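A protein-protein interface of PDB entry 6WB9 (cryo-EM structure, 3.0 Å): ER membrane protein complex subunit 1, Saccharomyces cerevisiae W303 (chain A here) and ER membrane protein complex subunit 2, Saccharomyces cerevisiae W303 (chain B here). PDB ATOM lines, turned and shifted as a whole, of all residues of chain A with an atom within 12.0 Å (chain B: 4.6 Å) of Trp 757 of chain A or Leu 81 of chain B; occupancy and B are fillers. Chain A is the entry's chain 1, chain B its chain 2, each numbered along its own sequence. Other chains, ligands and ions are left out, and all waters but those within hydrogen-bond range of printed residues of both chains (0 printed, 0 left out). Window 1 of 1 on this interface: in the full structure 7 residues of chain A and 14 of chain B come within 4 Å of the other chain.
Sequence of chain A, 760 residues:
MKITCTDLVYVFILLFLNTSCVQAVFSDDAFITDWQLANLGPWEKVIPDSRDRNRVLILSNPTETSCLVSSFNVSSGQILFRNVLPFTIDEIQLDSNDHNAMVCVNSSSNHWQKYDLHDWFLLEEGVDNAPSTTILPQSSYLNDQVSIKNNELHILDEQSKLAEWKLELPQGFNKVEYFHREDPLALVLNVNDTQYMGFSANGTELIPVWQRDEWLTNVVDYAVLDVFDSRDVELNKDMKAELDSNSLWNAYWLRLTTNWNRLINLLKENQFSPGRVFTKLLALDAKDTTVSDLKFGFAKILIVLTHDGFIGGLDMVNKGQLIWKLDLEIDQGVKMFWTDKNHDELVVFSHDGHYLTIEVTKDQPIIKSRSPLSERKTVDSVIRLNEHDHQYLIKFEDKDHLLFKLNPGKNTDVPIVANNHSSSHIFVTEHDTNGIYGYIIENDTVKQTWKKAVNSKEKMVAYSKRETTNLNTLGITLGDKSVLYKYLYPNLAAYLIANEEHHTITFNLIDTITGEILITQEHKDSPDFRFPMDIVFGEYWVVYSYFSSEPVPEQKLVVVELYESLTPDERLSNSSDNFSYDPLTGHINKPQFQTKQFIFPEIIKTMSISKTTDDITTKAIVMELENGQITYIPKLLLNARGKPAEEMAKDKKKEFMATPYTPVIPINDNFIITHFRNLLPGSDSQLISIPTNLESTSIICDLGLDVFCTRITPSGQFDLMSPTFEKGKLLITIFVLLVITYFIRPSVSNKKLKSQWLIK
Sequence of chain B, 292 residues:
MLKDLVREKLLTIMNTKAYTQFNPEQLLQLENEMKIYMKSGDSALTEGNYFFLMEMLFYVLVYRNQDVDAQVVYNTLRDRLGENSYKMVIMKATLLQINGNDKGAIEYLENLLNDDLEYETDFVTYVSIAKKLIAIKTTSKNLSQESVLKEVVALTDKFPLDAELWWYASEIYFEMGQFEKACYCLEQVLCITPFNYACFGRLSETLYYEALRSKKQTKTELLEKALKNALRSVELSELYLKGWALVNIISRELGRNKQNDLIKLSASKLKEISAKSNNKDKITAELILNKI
The side-chain amide oxygen of Asn 750 of chain A sits at hydrogen-bond distance from the guanidinium group of Arg 80 of chain B, at 2.4 Å.
The backbone carbonyl oxygen of Gln 756 of chain A lies within hydrogen-bond range of the side-chain amino group of Lys 87 of chain B (3.5 Å).
OG of Ser 85 of chain B sits at hydrogen-bond distance from N of Lys 87 of chain B, at 3.3 Å.
The side-chain hydroxyl (OG) of Ser 85 of chain B is in hydrogen-bond range of the backbone NH (N) of Met 88 of chain B.
OH of Tyr 86 of chain B is in hydrogen-bond range of NZ of Lys 87 of chain B (2.8 Å).
Leu 753 of chain A touches Phe 51 of chain B.
CD2 of Leu 753 of chain A touches CZ of Arg 80 of chain B, 3.5 Å away.
CD2 of Leu 753 of chain A touches CD2 of Leu 81 of chain B (3.8 Å).
NE1 of Trp 757 of chain A touches CE1 of Phe 52 of chain B, at 3.3 Å.
Trp 757 of chain A touches Leu 77 of chain B (CH2 to CD2, 3.7 Å).
Leu 81 of chain B touches Trp 757 of chain A.
CB of Ser 85 of chain B touches O of Trp 757 of chain A (3.3 Å).
CE1 of Tyr 86 of chain B touches O of Trp 757 of chain A, 3.5 Å away.
CD2 of Leu 758 of chain A touches N of Ser 85 of chain B (3.6 Å).
Tyr 86 of chain B touches Ile 759 of chain A.
Trp 757 of chain A touches nine residues of chain B.
Leu 81 of chain B touches just these residues of chain A: Leu 753 (3.8 Å) and Trp 757 (3.5 Å).
Phe 52 of chain B touches just these residues of chain A: Gln 756 and Trp 757.
Leu 77 of chain B touches just one residue of chain A: Trp 757.
Arg 80 of chain B touches just these residues of chain A: Asn 750 and Leu 753.
No residue of chain A comes within 4 Å of Gly 82 of chain B.
Printed residues of chain A within 4 Å of Ser 85 of chain B: Trp 757 and Leu 758.
Of the printed residues of chain A, Lys 87 of chain B touches Gln 756 and Trp 757.
Of the printed residues of chain A, Met 88 of chain B touches Trp 757 (3.7 Å).
Of the printed residues of chain B, Ile 759 of chain A touches Tyr 86.
Of the printed residues of chain B, Asn 750 of chain A touches Arg 80 (2.4 Å).
Of the printed residues of chain B, Gln 756 of chain A touches Gly 48, Phe 52 and Lys 87.
Glu 83 of chain B touches none of the printed residues of chain A.
Val 748 of chain A touches none of the printed residues of chain B.
The nearest residue of chain B that does not touch Trp 757 of chain A is Gly 48 of chain B (4.5 Å).
The nearest residue of chain A that does not touch Leu 81 of chain B is Lys 754 of chain A (5.2 Å).
Printed residues of chain A that touch a printed residue of chain B: Asn 750, Leu 753, Gln 756, Trp 757, Leu 758 and Ile 759.
Hydrophobic or aromatic side chains of chain A within 4 Å of the printed part of chain B: Leu 753, Trp 757 and Leu 758.
Of the 15 printed residues of chain B, 11 touch a printed residue of chain A.
Among the printed residues, no Asp or Glu carboxylate lies within 4 Å of a Lys or Arg side-chain nitrogen of the other chain.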
ATOM      1  N   PRO A 746     -12.742 -27.016 -29.776  1.00  0.00           N
ATOM      2  CA  PRO A 746     -11.916 -25.883 -29.316  1.00  0.00           C
ATOM      3  C   PRO A 746     -11.086 -26.181 -28.078  1.00  0.00           C
ATOM      4  O   PRO A 746     -10.044 -25.544 -27.890  1.00  0.00           O
ATOM      5  CB  PRO A 746     -12.944 -24.774 -29.047  1.00  0.00           C
ATOM      6  CG  PRO A 746     -14.207 -25.479 -28.834  1.00  0.00           C
ATOM      7  CD  PRO A 746     -14.164 -26.610 -29.798  1.00  0.00           C
ATOM      8  N   SER A 747     -11.489 -27.150 -27.254  1.00  0.00           N
ATOM      9  CA  SER A 747     -10.654 -27.558 -26.127  1.00  0.00           C
ATOM     10  C   SER A 747      -9.368 -28.226 -26.602  1.00  0.00           C
ATOM     11  O   SER A 747      -8.295 -27.987 -26.040  1.00  0.00           O
ATOM     12  CB  SER A 747     -11.435 -28.494 -25.209  1.00  0.00           C
ATOM     13  OG  SER A 747     -10.642 -28.904 -24.112  1.00  0.00           O
ATOM     14  N   VAL A 748      -9.450 -29.031 -27.663  1.00  0.00           N
ATOM     15  CA  VAL A 748      -8.254 -29.651 -28.230  1.00  0.00           C
ATOM     16  C   VAL A 748      -7.411 -28.612 -28.959  1.00  0.00           C
ATOM     17  O   VAL A 748      -6.175 -28.616 -28.864  1.00  0.00           O
ATOM     18  CB  VAL A 748      -8.653 -30.818 -29.151  1.00  0.00           C
ATOM     19  CG1 VAL A 748      -7.429 -31.487 -29.752  1.00  0.00           C
ATOM     20  CG2 VAL A 748      -9.461 -31.823 -28.376  1.00  0.00           C
ATOM     21  N   SER A 749      -8.062 -27.692 -29.679  1.00  0.00           N
ATOM     22  CA  SER A 749      -7.347 -26.625 -30.371  1.00  0.00           C
ATOM     23  C   SER A 749      -6.677 -25.649 -29.412  1.00  0.00           C
ATOM     24  O   SER A 749      -5.712 -24.984 -29.800  1.00  0.00           O
ATOM     25  CB  SER A 749      -8.301 -25.867 -31.292  1.00  0.00           C
ATOM     26  OG  SER A 749      -7.673 -24.721 -31.836  1.00  0.00           O
ATOM     27  N   ASN A 750      -7.166 -25.547 -28.176  1.00  0.00           N
ATOM     28  CA  ASN A 750      -6.501 -24.759 -27.149  1.00  0.00           C
ATOM     29  C   ASN A 750      -5.428 -25.548 -26.414  1.00  0.00           C
ATOM     30  O   ASN A 750      -4.400 -24.974 -26.036  1.00  0.00           O
ATOM     31  CB  ASN A 750      -7.536 -24.231 -26.151  1.00  0.00           C
ATOM     32  CG  ASN A 750      -6.923 -23.349 -25.088  1.00  0.00           C
ATOM     33  OD1 ASN A 750      -6.627 -22.180 -25.329  1.00  0.00           O
ATOM     34  ND2 ASN A 750      -6.738 -23.903 -23.896  1.00  0.00           N
ATOM     35  N   LYS A 751      -5.624 -26.856 -26.224  1.00  0.00           N
ATOM     36  CA  LYS A 751      -4.622 -27.652 -25.525  1.00  0.00           C
ATOM     37  C   LYS A 751      -3.382 -27.881 -26.379  1.00  0.00           C
ATOM     38  O   LYS A 751      -2.266 -27.912 -25.847  1.00  0.00           O
ATOM     39  CB  LYS A 751      -5.214 -28.989 -25.091  1.00  0.00           C
ATOM     40  CG  LYS A 751      -4.399 -29.687 -24.025  1.00  0.00           C
ATOM     41  CD  LYS A 751      -4.076 -31.109 -24.420  1.00  0.00           C
ATOM     42  CE  LYS A 751      -3.277 -31.797 -23.334  1.00  0.00           C
ATOM     43  NZ  LYS A 751      -1.976 -31.122 -23.094  1.00  0.00           N
ATOM     44  N   LYS A 752      -3.548 -28.026 -27.698  1.00  0.00           N
ATOM     45  CA  LYS A 752      -2.383 -28.129 -28.575  1.00  0.00           C
ATOM     46  C   LYS A 752      -1.614 -26.815 -28.623  1.00  0.00           C
ATOM     47  O   LYS A 752      -0.380 -26.813 -28.690  1.00  0.00           O
ATOM     48  CB  LYS A 752      -2.808 -28.552 -29.978  1.00  0.00           C
ATOM     49  CG  LYS A 752      -3.377 -29.957 -30.063  1.00  0.00           C
ATOM     50  CD  LYS A 752      -3.550 -30.394 -31.508  1.00  0.00           C
ATOM     51  CE  LYS A 752      -4.417 -29.420 -32.289  1.00  0.00           C
ATOM     52  NZ  LYS A 752      -4.484 -29.779 -33.731  1.00  0.00           N
ATOM     53  N   LEU A 753      -2.326 -25.688 -28.553  1.00  0.00           N
ATOM     54  CA  LEU A 753      -1.669 -24.387 -28.509  1.00  0.00           C
ATOM     55  C   LEU A 753      -0.925 -24.185 -27.194  1.00  0.00           C
ATOM     56  O   LEU A 753       0.167 -23.601 -27.172  1.00  0.00           O
ATOM     57  CB  LEU A 753      -2.704 -23.286 -28.719  1.00  0.00           C
ATOM     58  CG  LEU A 753      -2.200 -21.850 -28.775  1.00  0.00           C
ATOM     59  CD1 LEU A 753      -1.293 -21.667 -29.961  1.00  0.00           C
ATOM     60  CD2 LEU A 753      -3.366 -20.900 -28.855  1.00  0.00           C
ATOM     61  N   LYS A 754      -1.497 -24.673 -26.090  1.00  0.00           N
ATOM     62  CA  LYS A 754      -0.804 -24.625 -24.806  1.00  0.00           C
ATOM     63  C   LYS A 754       0.416 -25.536 -24.800  1.00  0.00           C
ATOM     64  O   LYS A 754       1.427 -25.220 -24.166  1.00  0.00           O
ATOM     65  CB  LYS A 754      -1.759 -25.010 -23.680  1.00  0.00           C
ATOM     66  CG  LYS A 754      -2.756 -23.933 -23.304  1.00  0.00           C
ATOM     67  CD  LYS A 754      -3.776 -24.450 -22.299  1.00  0.00           C
ATOM     68  CE  LYS A 754      -3.113 -25.023 -21.052  1.00  0.00           C
ATOM     69  NZ  LYS A 754      -3.176 -26.512 -21.017  1.00  0.00           N
ATOM     70  N   SER A 755       0.340 -26.674 -25.493  1.00  0.00           N
ATOM     71  CA  SER A 755       1.516 -27.525 -25.636  1.00  0.00           C
ATOM     72  C   SER A 755       2.582 -26.866 -26.501  1.00  0.00           C
ATOM     73  O   SER A 755       3.779 -27.080 -26.278  1.00  0.00           O
ATOM     74  CB  SER A 755       1.115 -28.876 -26.224  1.00  0.00           C
ATOM     75  OG  SER A 755       2.253 -29.673 -26.496  1.00  0.00           O
ATOM     76  N   GLN A 756       2.170 -26.066 -27.486  1.00  0.00           N
ATOM     77  CA  GLN A 756       3.138 -25.354 -28.312  1.00  0.00           C
ATOM     78  C   GLN A 756       3.791 -24.200 -27.562  1.00  0.00           C
ATOM     79  O   GLN A 756       4.955 -23.879 -27.825  1.00  0.00           O
ATOM     80  CB  GLN A 756       2.473 -24.830 -29.582  1.00  0.00           C
ATOM     81  CG  GLN A 756       2.133 -25.896 -30.600  1.00  0.00           C
ATOM     82  CD  GLN A 756       1.535 -25.319 -31.861  1.00  0.00           C
ATOM     83  OE1 GLN A 756       2.187 -24.567 -32.580  1.00  0.00           O
ATOM     84  NE2 GLN A 756       0.281 -25.661 -32.134  1.00  0.00           N
ATOM     85  N   TRP A 757       3.073 -23.562 -26.639  1.00  0.00           N
ATOM     86  CA  TRP A 757       3.585 -22.355 -25.994  1.00  0.00           C
ATOM     87  C   TRP A 757       4.139 -22.589 -24.594  1.00  0.00           C
ATOM     88  O   TRP A 757       5.242 -22.126 -24.296  1.00  0.00           O
ATOM     89  CB  TRP A 757       2.495 -21.284 -25.949  1.00  0.00           C
ATOM     90  CG  TRP A 757       2.362 -20.544 -27.229  1.00  0.00           C
ATOM     91  CD1 TRP A 757       1.830 -21.014 -28.389  1.00  0.00           C
ATOM     92  CD2 TRP A 757       2.772 -19.200 -27.490  1.00  0.00           C
ATOM     93  NE1 TRP A 757       1.880 -20.046 -29.358  1.00  0.00           N
ATOM     94  CE2 TRP A 757       2.453 -18.920 -28.829  1.00  0.00           C
ATOM     95  CE3 TRP A 757       3.372 -18.203 -26.719  1.00  0.00           C
ATOM     96  CZ2 TRP A 757       2.718 -17.688 -29.417  1.00  0.00           C
ATOM     97  CZ3 TRP A 757       3.628 -16.980 -27.304  1.00  0.00           C
ATOM     98  CH2 TRP A 757       3.306 -16.733 -28.638  1.00  0.00           C
ATOM     99  N   LEU A 758       3.395 -23.276 -23.718  1.00  0.00           N
ATOM    100  CA  LEU A 758       3.839 -23.421 -22.331  1.00  0.00           C
ATOM    101  C   LEU A 758       5.037 -24.355 -22.225  1.00  0.00           C
ATOM    102  O   LEU A 758       5.973 -24.088 -21.463  1.00  0.00           O
ATOM    103  CB  LEU A 758       2.703 -23.934 -21.440  1.00  0.00           C
ATOM    104  CG  LEU A 758       1.298 -23.325 -21.439  1.00  0.00           C
ATOM    105  CD1 LEU A 758       0.468 -23.984 -20.353  1.00  0.00           C
ATOM    106  CD2 LEU A 758       1.309 -21.829 -21.248  1.00  0.00           C
ATOM    107  N   ILE A 759       5.027 -25.448 -22.978  1.00  0.00           N
ATOM    108  CA  ILE A 759       6.117 -26.410 -22.936  1.00  0.00           C
ATOM    109  C   ILE A 759       7.233 -25.966 -23.868  1.00  0.00           C
ATOM    110  O   ILE A 759       7.879 -24.947 -23.632  1.00  0.00           O
ATOM    111  CB  ILE A 759       5.626 -27.824 -23.298  1.00  0.00           C
ATOM    112  CG1 ILE A 759       4.438 -28.218 -22.416  1.00  0.00           C
ATOM    113  CG2 ILE A 759       6.757 -28.833 -23.159  1.00  0.00           C
ATOM    114  CD1 ILE A 759       3.846 -29.570 -22.749  1.00  0.00           C
ATOM    115  N   GLY B  48      -1.519 -22.239 -34.092  1.00  0.00           N
ATOM    116  CA  GLY B  48      -0.211 -22.106 -33.470  1.00  0.00           C
ATOM    117  C   GLY B  48       0.767 -21.331 -34.328  1.00  0.00           C
ATOM    118  O   GLY B  48       1.539 -20.515 -33.820  1.00  0.00           O
ATOM    119  N   PHE B  51      -0.186 -17.612 -33.936  1.00  0.00           N
ATOM    120  CA  PHE B  51       0.302 -16.934 -32.739  1.00  0.00           C
ATOM    121  C   PHE B  51       1.823 -16.867 -32.697  1.00  0.00           C
ATOM    122  O   PHE B  51       2.378 -15.930 -32.112  1.00  0.00           O
ATOM    123  CB  PHE B  51      -0.275 -17.598 -31.494  1.00  0.00           C
ATOM    124  CG  PHE B  51      -1.741 -17.353 -31.336  1.00  0.00           C
ATOM    125  CD1 PHE B  51      -2.215 -16.062 -31.190  1.00  0.00           C
ATOM    126  CD2 PHE B  51      -2.647 -18.394 -31.374  1.00  0.00           C
ATOM    127  CE1 PHE B  51      -3.560 -15.814 -31.068  1.00  0.00           C
ATOM    128  CE2 PHE B  51      -3.996 -18.152 -31.252  1.00  0.00           C
ATOM    129  CZ  PHE B  51      -4.453 -16.861 -31.108  1.00  0.00           C
ATOM    130  N   PHE B  52       2.510 -17.796 -33.364  1.00  0.00           N
ATOM    131  CA  PHE B  52       3.954 -17.665 -33.526  1.00  0.00           C
ATOM    132  C   PHE B  52       4.309 -16.504 -34.450  1.00  0.00           C
ATOM    133  O   PHE B  52       5.260 -15.756 -34.183  1.00  0.00           O
ATOM    134  CB  PHE B  52       4.531 -18.970 -34.053  1.00  0.00           C
ATOM    135  CG  PHE B  52       4.633 -20.053 -33.024  1.00  0.00           C
ATOM    136  CD1 PHE B  52       4.754 -19.744 -31.682  1.00  0.00           C
ATOM    137  CD2 PHE B  52       4.615 -21.385 -33.402  1.00  0.00           C
ATOM    138  CE1 PHE B  52       4.849 -20.741 -30.737  1.00  0.00           C
ATOM    139  CE2 PHE B  52       4.708 -22.386 -32.462  1.00  0.00           C
ATOM    140  CZ  PHE B  52       4.827 -22.063 -31.127  1.00  0.00           C
ATOM    141  N   GLU B  55       3.839 -13.404 -32.395  1.00  0.00           N
ATOM    142  CA  GLU B  55       5.011 -13.157 -31.553  1.00  0.00           C
ATOM    143  C   GLU B  55       6.157 -12.555 -32.360  1.00  0.00           C
ATOM    144  O   GLU B  55       6.835 -11.619 -31.904  1.00  0.00           O
ATOM    145  CB  GLU B  55       5.452 -14.459 -30.889  1.00  0.00           C
ATOM    146  CG  GLU B  55       6.736 -14.349 -30.095  1.00  0.00           C
ATOM    147  CD  GLU B  55       7.373 -15.694 -29.831  1.00  0.00           C
ATOM    148  OE1 GLU B  55       6.993 -16.674 -30.505  1.00  0.00           O
ATOM    149  OE2 GLU B  55       8.254 -15.771 -28.953  1.00  0.00           O
ATOM    150  N   LEU B  77      -2.128 -11.402 -27.511  1.00  0.00           N
ATOM    151  CA  LEU B  77      -1.549 -12.694 -27.151  1.00  0.00           C
ATOM    152  C   LEU B  77      -1.777 -13.037 -25.682  1.00  0.00           C
ATOM    153  O   LEU B  77      -1.879 -14.220 -25.338  1.00  0.00           O
ATOM    154  CB  LEU B  77      -0.059 -12.705 -27.489  1.00  0.00           C
ATOM    155  CG  LEU B  77       0.231 -13.064 -28.946  1.00  0.00           C
ATOM    156  CD1 LEU B  77       1.466 -12.366 -29.457  1.00  0.00           C
ATOM    157  CD2 LEU B  77       0.378 -14.563 -29.091  1.00  0.00           C
ATOM    158  N   ARG B  78      -1.863 -12.033 -24.808  1.00  0.00           N
ATOM    159  CA  ARG B  78      -2.217 -12.285 -23.415  1.00  0.00           C
ATOM    160  C   ARG B  78      -3.694 -12.627 -23.273  1.00  0.00           C
ATOM    161  O   ARG B  78      -4.059 -13.462 -22.437  1.00  0.00           O
ATOM    162  CB  ARG B  78      -1.856 -11.069 -22.557  1.00  0.00           C
ATOM    163  CG  ARG B  78      -2.152 -11.221 -21.070  1.00  0.00           C
ATOM    164  CD  ARG B  78      -1.610 -10.057 -20.264  1.00  0.00           C
ATOM    165  NE  ARG B  78      -2.003  -8.769 -20.822  1.00  0.00           N
ATOM    166  CZ  ARG B  78      -1.675  -7.597 -20.289  1.00  0.00           C
ATOM    167  NH1 ARG B  78      -2.071  -6.470 -20.865  1.00  0.00           N
ATOM    168  NH2 ARG B  78      -0.953  -7.551 -19.178  1.00  0.00           N
ATOM    169  N   ASP B  79      -4.553 -12.009 -24.091  1.00  0.00           N
ATOM    170  CA  ASP B  79      -5.970 -12.355 -24.089  1.00  0.00           C
ATOM    171  C   ASP B  79      -6.208 -13.765 -24.608  1.00  0.00           C
ATOM    172  O   ASP B  79      -7.216 -14.388 -24.260  1.00  0.00           O
ATOM    173  CB  ASP B  79      -6.763 -11.348 -24.922  1.00  0.00           C
ATOM    174  CG  ASP B  79      -6.879  -9.998 -24.248  1.00  0.00           C
ATOM    175  OD1 ASP B  79      -6.870  -9.953 -23.000  1.00  0.00           O
ATOM    176  OD2 ASP B  79      -6.973  -8.981 -24.968  1.00  0.00           O
ATOM    177  N   ARG B  80      -5.302 -14.286 -25.434  1.00  0.00           N
ATOM    178  CA  ARG B  80      -5.428 -15.690 -25.808  1.00  0.00           C
ATOM    179  C   ARG B  80      -4.717 -16.626 -24.834  1.00  0.00           C
ATOM    180  O   ARG B  80      -5.303 -17.615 -24.385  1.00  0.00           O
ATOM    181  CB  ARG B  80      -4.893 -15.920 -27.218  1.00  0.00           C
ATOM    182  CG  ARG B  80      -5.082 -17.345 -27.684  1.00  0.00           C
ATOM    183  CD  ARG B  80      -6.553 -17.686 -27.803  1.00  0.00           C
ATOM    184  NE  ARG B  80      -6.776 -18.868 -28.627  1.00  0.00           N
ATOM    185  CZ  ARG B  80      -6.754 -20.112 -28.167  1.00  0.00           C
ATOM    186  NH1 ARG B  80      -6.514 -20.341 -26.884  1.00  0.00           N
ATOM    187  NH2 ARG B  80      -6.967 -21.128 -28.991  1.00  0.00           N
ATOM    188  N   LEU B  81      -3.463 -16.333 -24.496  1.00  0.00           N
ATOM    189  CA  LEU B  81      -2.609 -17.271 -23.773  1.00  0.00           C
ATOM    190  C   LEU B  81      -2.331 -16.880 -22.332  1.00  0.00           C
ATOM    191  O   LEU B  81      -2.290 -17.754 -21.463  1.00  0.00           O
ATOM    192  CB  LEU B  81      -1.276 -17.428 -24.509  1.00  0.00           C
ATOM    193  CG  LEU B  81      -1.397 -17.940 -25.941  1.00  0.00           C
ATOM    194  CD1 LEU B  81      -0.233 -17.457 -26.766  1.00  0.00           C
ATOM    195  CD2 LEU B  81      -1.465 -19.450 -25.948  1.00  0.00           C
ATOM    196  N   GLY B  82      -2.129 -15.598 -22.047  1.00  0.00           N
ATOM    197  CA  GLY B  82      -1.778 -15.166 -20.712  1.00  0.00           C
ATOM    198  C   GLY B  82      -0.285 -15.246 -20.457  1.00  0.00           C
ATOM    199  O   GLY B  82       0.487 -15.812 -21.229  1.00  0.00           O
ATOM    200  N   GLU B  83       0.126 -14.671 -19.331  1.00  0.00           N
ATOM    201  CA  GLU B  83       1.543 -14.577 -18.972  1.00  0.00           C
ATOM    202  C   GLU B  83       2.036 -15.830 -18.255  1.00  0.00           C
ATOM    203  O   GLU B  83       2.615 -15.757 -17.173  1.00  0.00           O
ATOM    204  CB  GLU B  83       1.769 -13.341 -18.114  1.00  0.00           C
ATOM    205  CG  GLU B  83       1.009 -12.113 -18.579  1.00  0.00           C
ATOM    206  CD  GLU B  83       0.993 -11.009 -17.539  1.00  0.00           C
ATOM    207  OE1 GLU B  83       1.092 -11.326 -16.335  1.00  0.00           O
ATOM    208  OE2 GLU B  83       0.885  -9.826 -17.923  1.00  0.00           O
ATOM    209  N   SER B  85       3.287 -18.901 -20.342  1.00  0.00           N
ATOM    210  CA  SER B  85       4.320 -19.546 -21.134  1.00  0.00           C
ATOM    211  C   SER B  85       5.636 -18.791 -20.995  1.00  0.00           C
ATOM    212  O   SER B  85       5.692 -17.679 -20.467  1.00  0.00           O
ATOM    213  CB  SER B  85       3.918 -19.608 -22.604  1.00  0.00           C
ATOM    214  OG  SER B  85       4.209 -18.390 -23.255  1.00  0.00           O
ATOM    215  N   TYR B  86       6.710 -19.408 -21.488  1.00  0.00           N
ATOM    216  CA  TYR B  86       8.003 -18.740 -21.430  1.00  0.00           C
ATOM    217  C   TYR B  86       8.084 -17.611 -22.447  1.00  0.00           C
ATOM    218  O   TYR B  86       8.685 -16.572 -22.165  1.00  0.00           O
ATOM    219  CB  TYR B  86       9.140 -19.744 -21.626  1.00  0.00           C
ATOM    220  CG  TYR B  86       9.293 -20.327 -23.015  1.00  0.00           C
ATOM    221  CD1 TYR B  86       8.529 -21.411 -23.424  1.00  0.00           C
ATOM    222  CD2 TYR B  86      10.229 -19.814 -23.903  1.00  0.00           C
ATOM    223  CE1 TYR B  86       8.677 -21.950 -24.684  1.00  0.00           C
ATOM    224  CE2 TYR B  86      10.388 -20.348 -25.162  1.00  0.00           C
ATOM    225  CZ  TYR B  86       9.609 -21.415 -25.546  1.00  0.00           C
ATOM    226  OH  TYR B  86       9.761 -21.952 -26.803  1.00  0.00           O
ATOM    227  N   LYS B  87       7.458 -17.784 -23.618  1.00  0.00           N
ATOM    228  CA  LYS B  87       7.517 -16.766 -24.665  1.00  0.00           C
ATOM    229  C   LYS B  87       6.795 -15.495 -24.247  1.00  0.00           C
ATOM    230  O   LYS B  87       7.277 -14.389 -24.509  1.00  0.00           O
ATOM    231  CB  LYS B  87       6.916 -17.299 -25.962  1.00  0.00           C
ATOM    232  CG  LYS B  87       7.581 -18.526 -26.539  1.00  0.00           C
ATOM    233  CD  LYS B  87       7.044 -18.806 -27.930  1.00  0.00           C
ATOM    234  CE  LYS B  87       7.634 -20.067 -28.517  1.00  0.00           C
ATOM    235  NZ  LYS B  87       7.222 -21.271 -27.753  1.00  0.00           N
ATOM    236  N   MET B  88       5.652 -15.633 -23.570  1.00  0.00           N
ATOM    237  CA  MET B  88       4.943 -14.466 -23.056  1.00  0.00           C
ATOM    238  C   MET B  88       5.719 -13.794 -21.931  1.00  0.00           C
ATOM    239  O   MET B  88       5.633 -12.574 -21.767  1.00  0.00           O
ATOM    240  CB  MET B  88       3.551 -14.872 -22.582  1.00  0.00           C
ATOM    241  CG  MET B  88       2.704 -15.495 -23.669  1.00  0.00           C
ATOM    242  SD  MET B  88       2.373 -14.333 -24.994  1.00  0.00           S
ATOM    243  CE  MET B  88       1.410 -13.133 -24.096  1.00  0.00           C
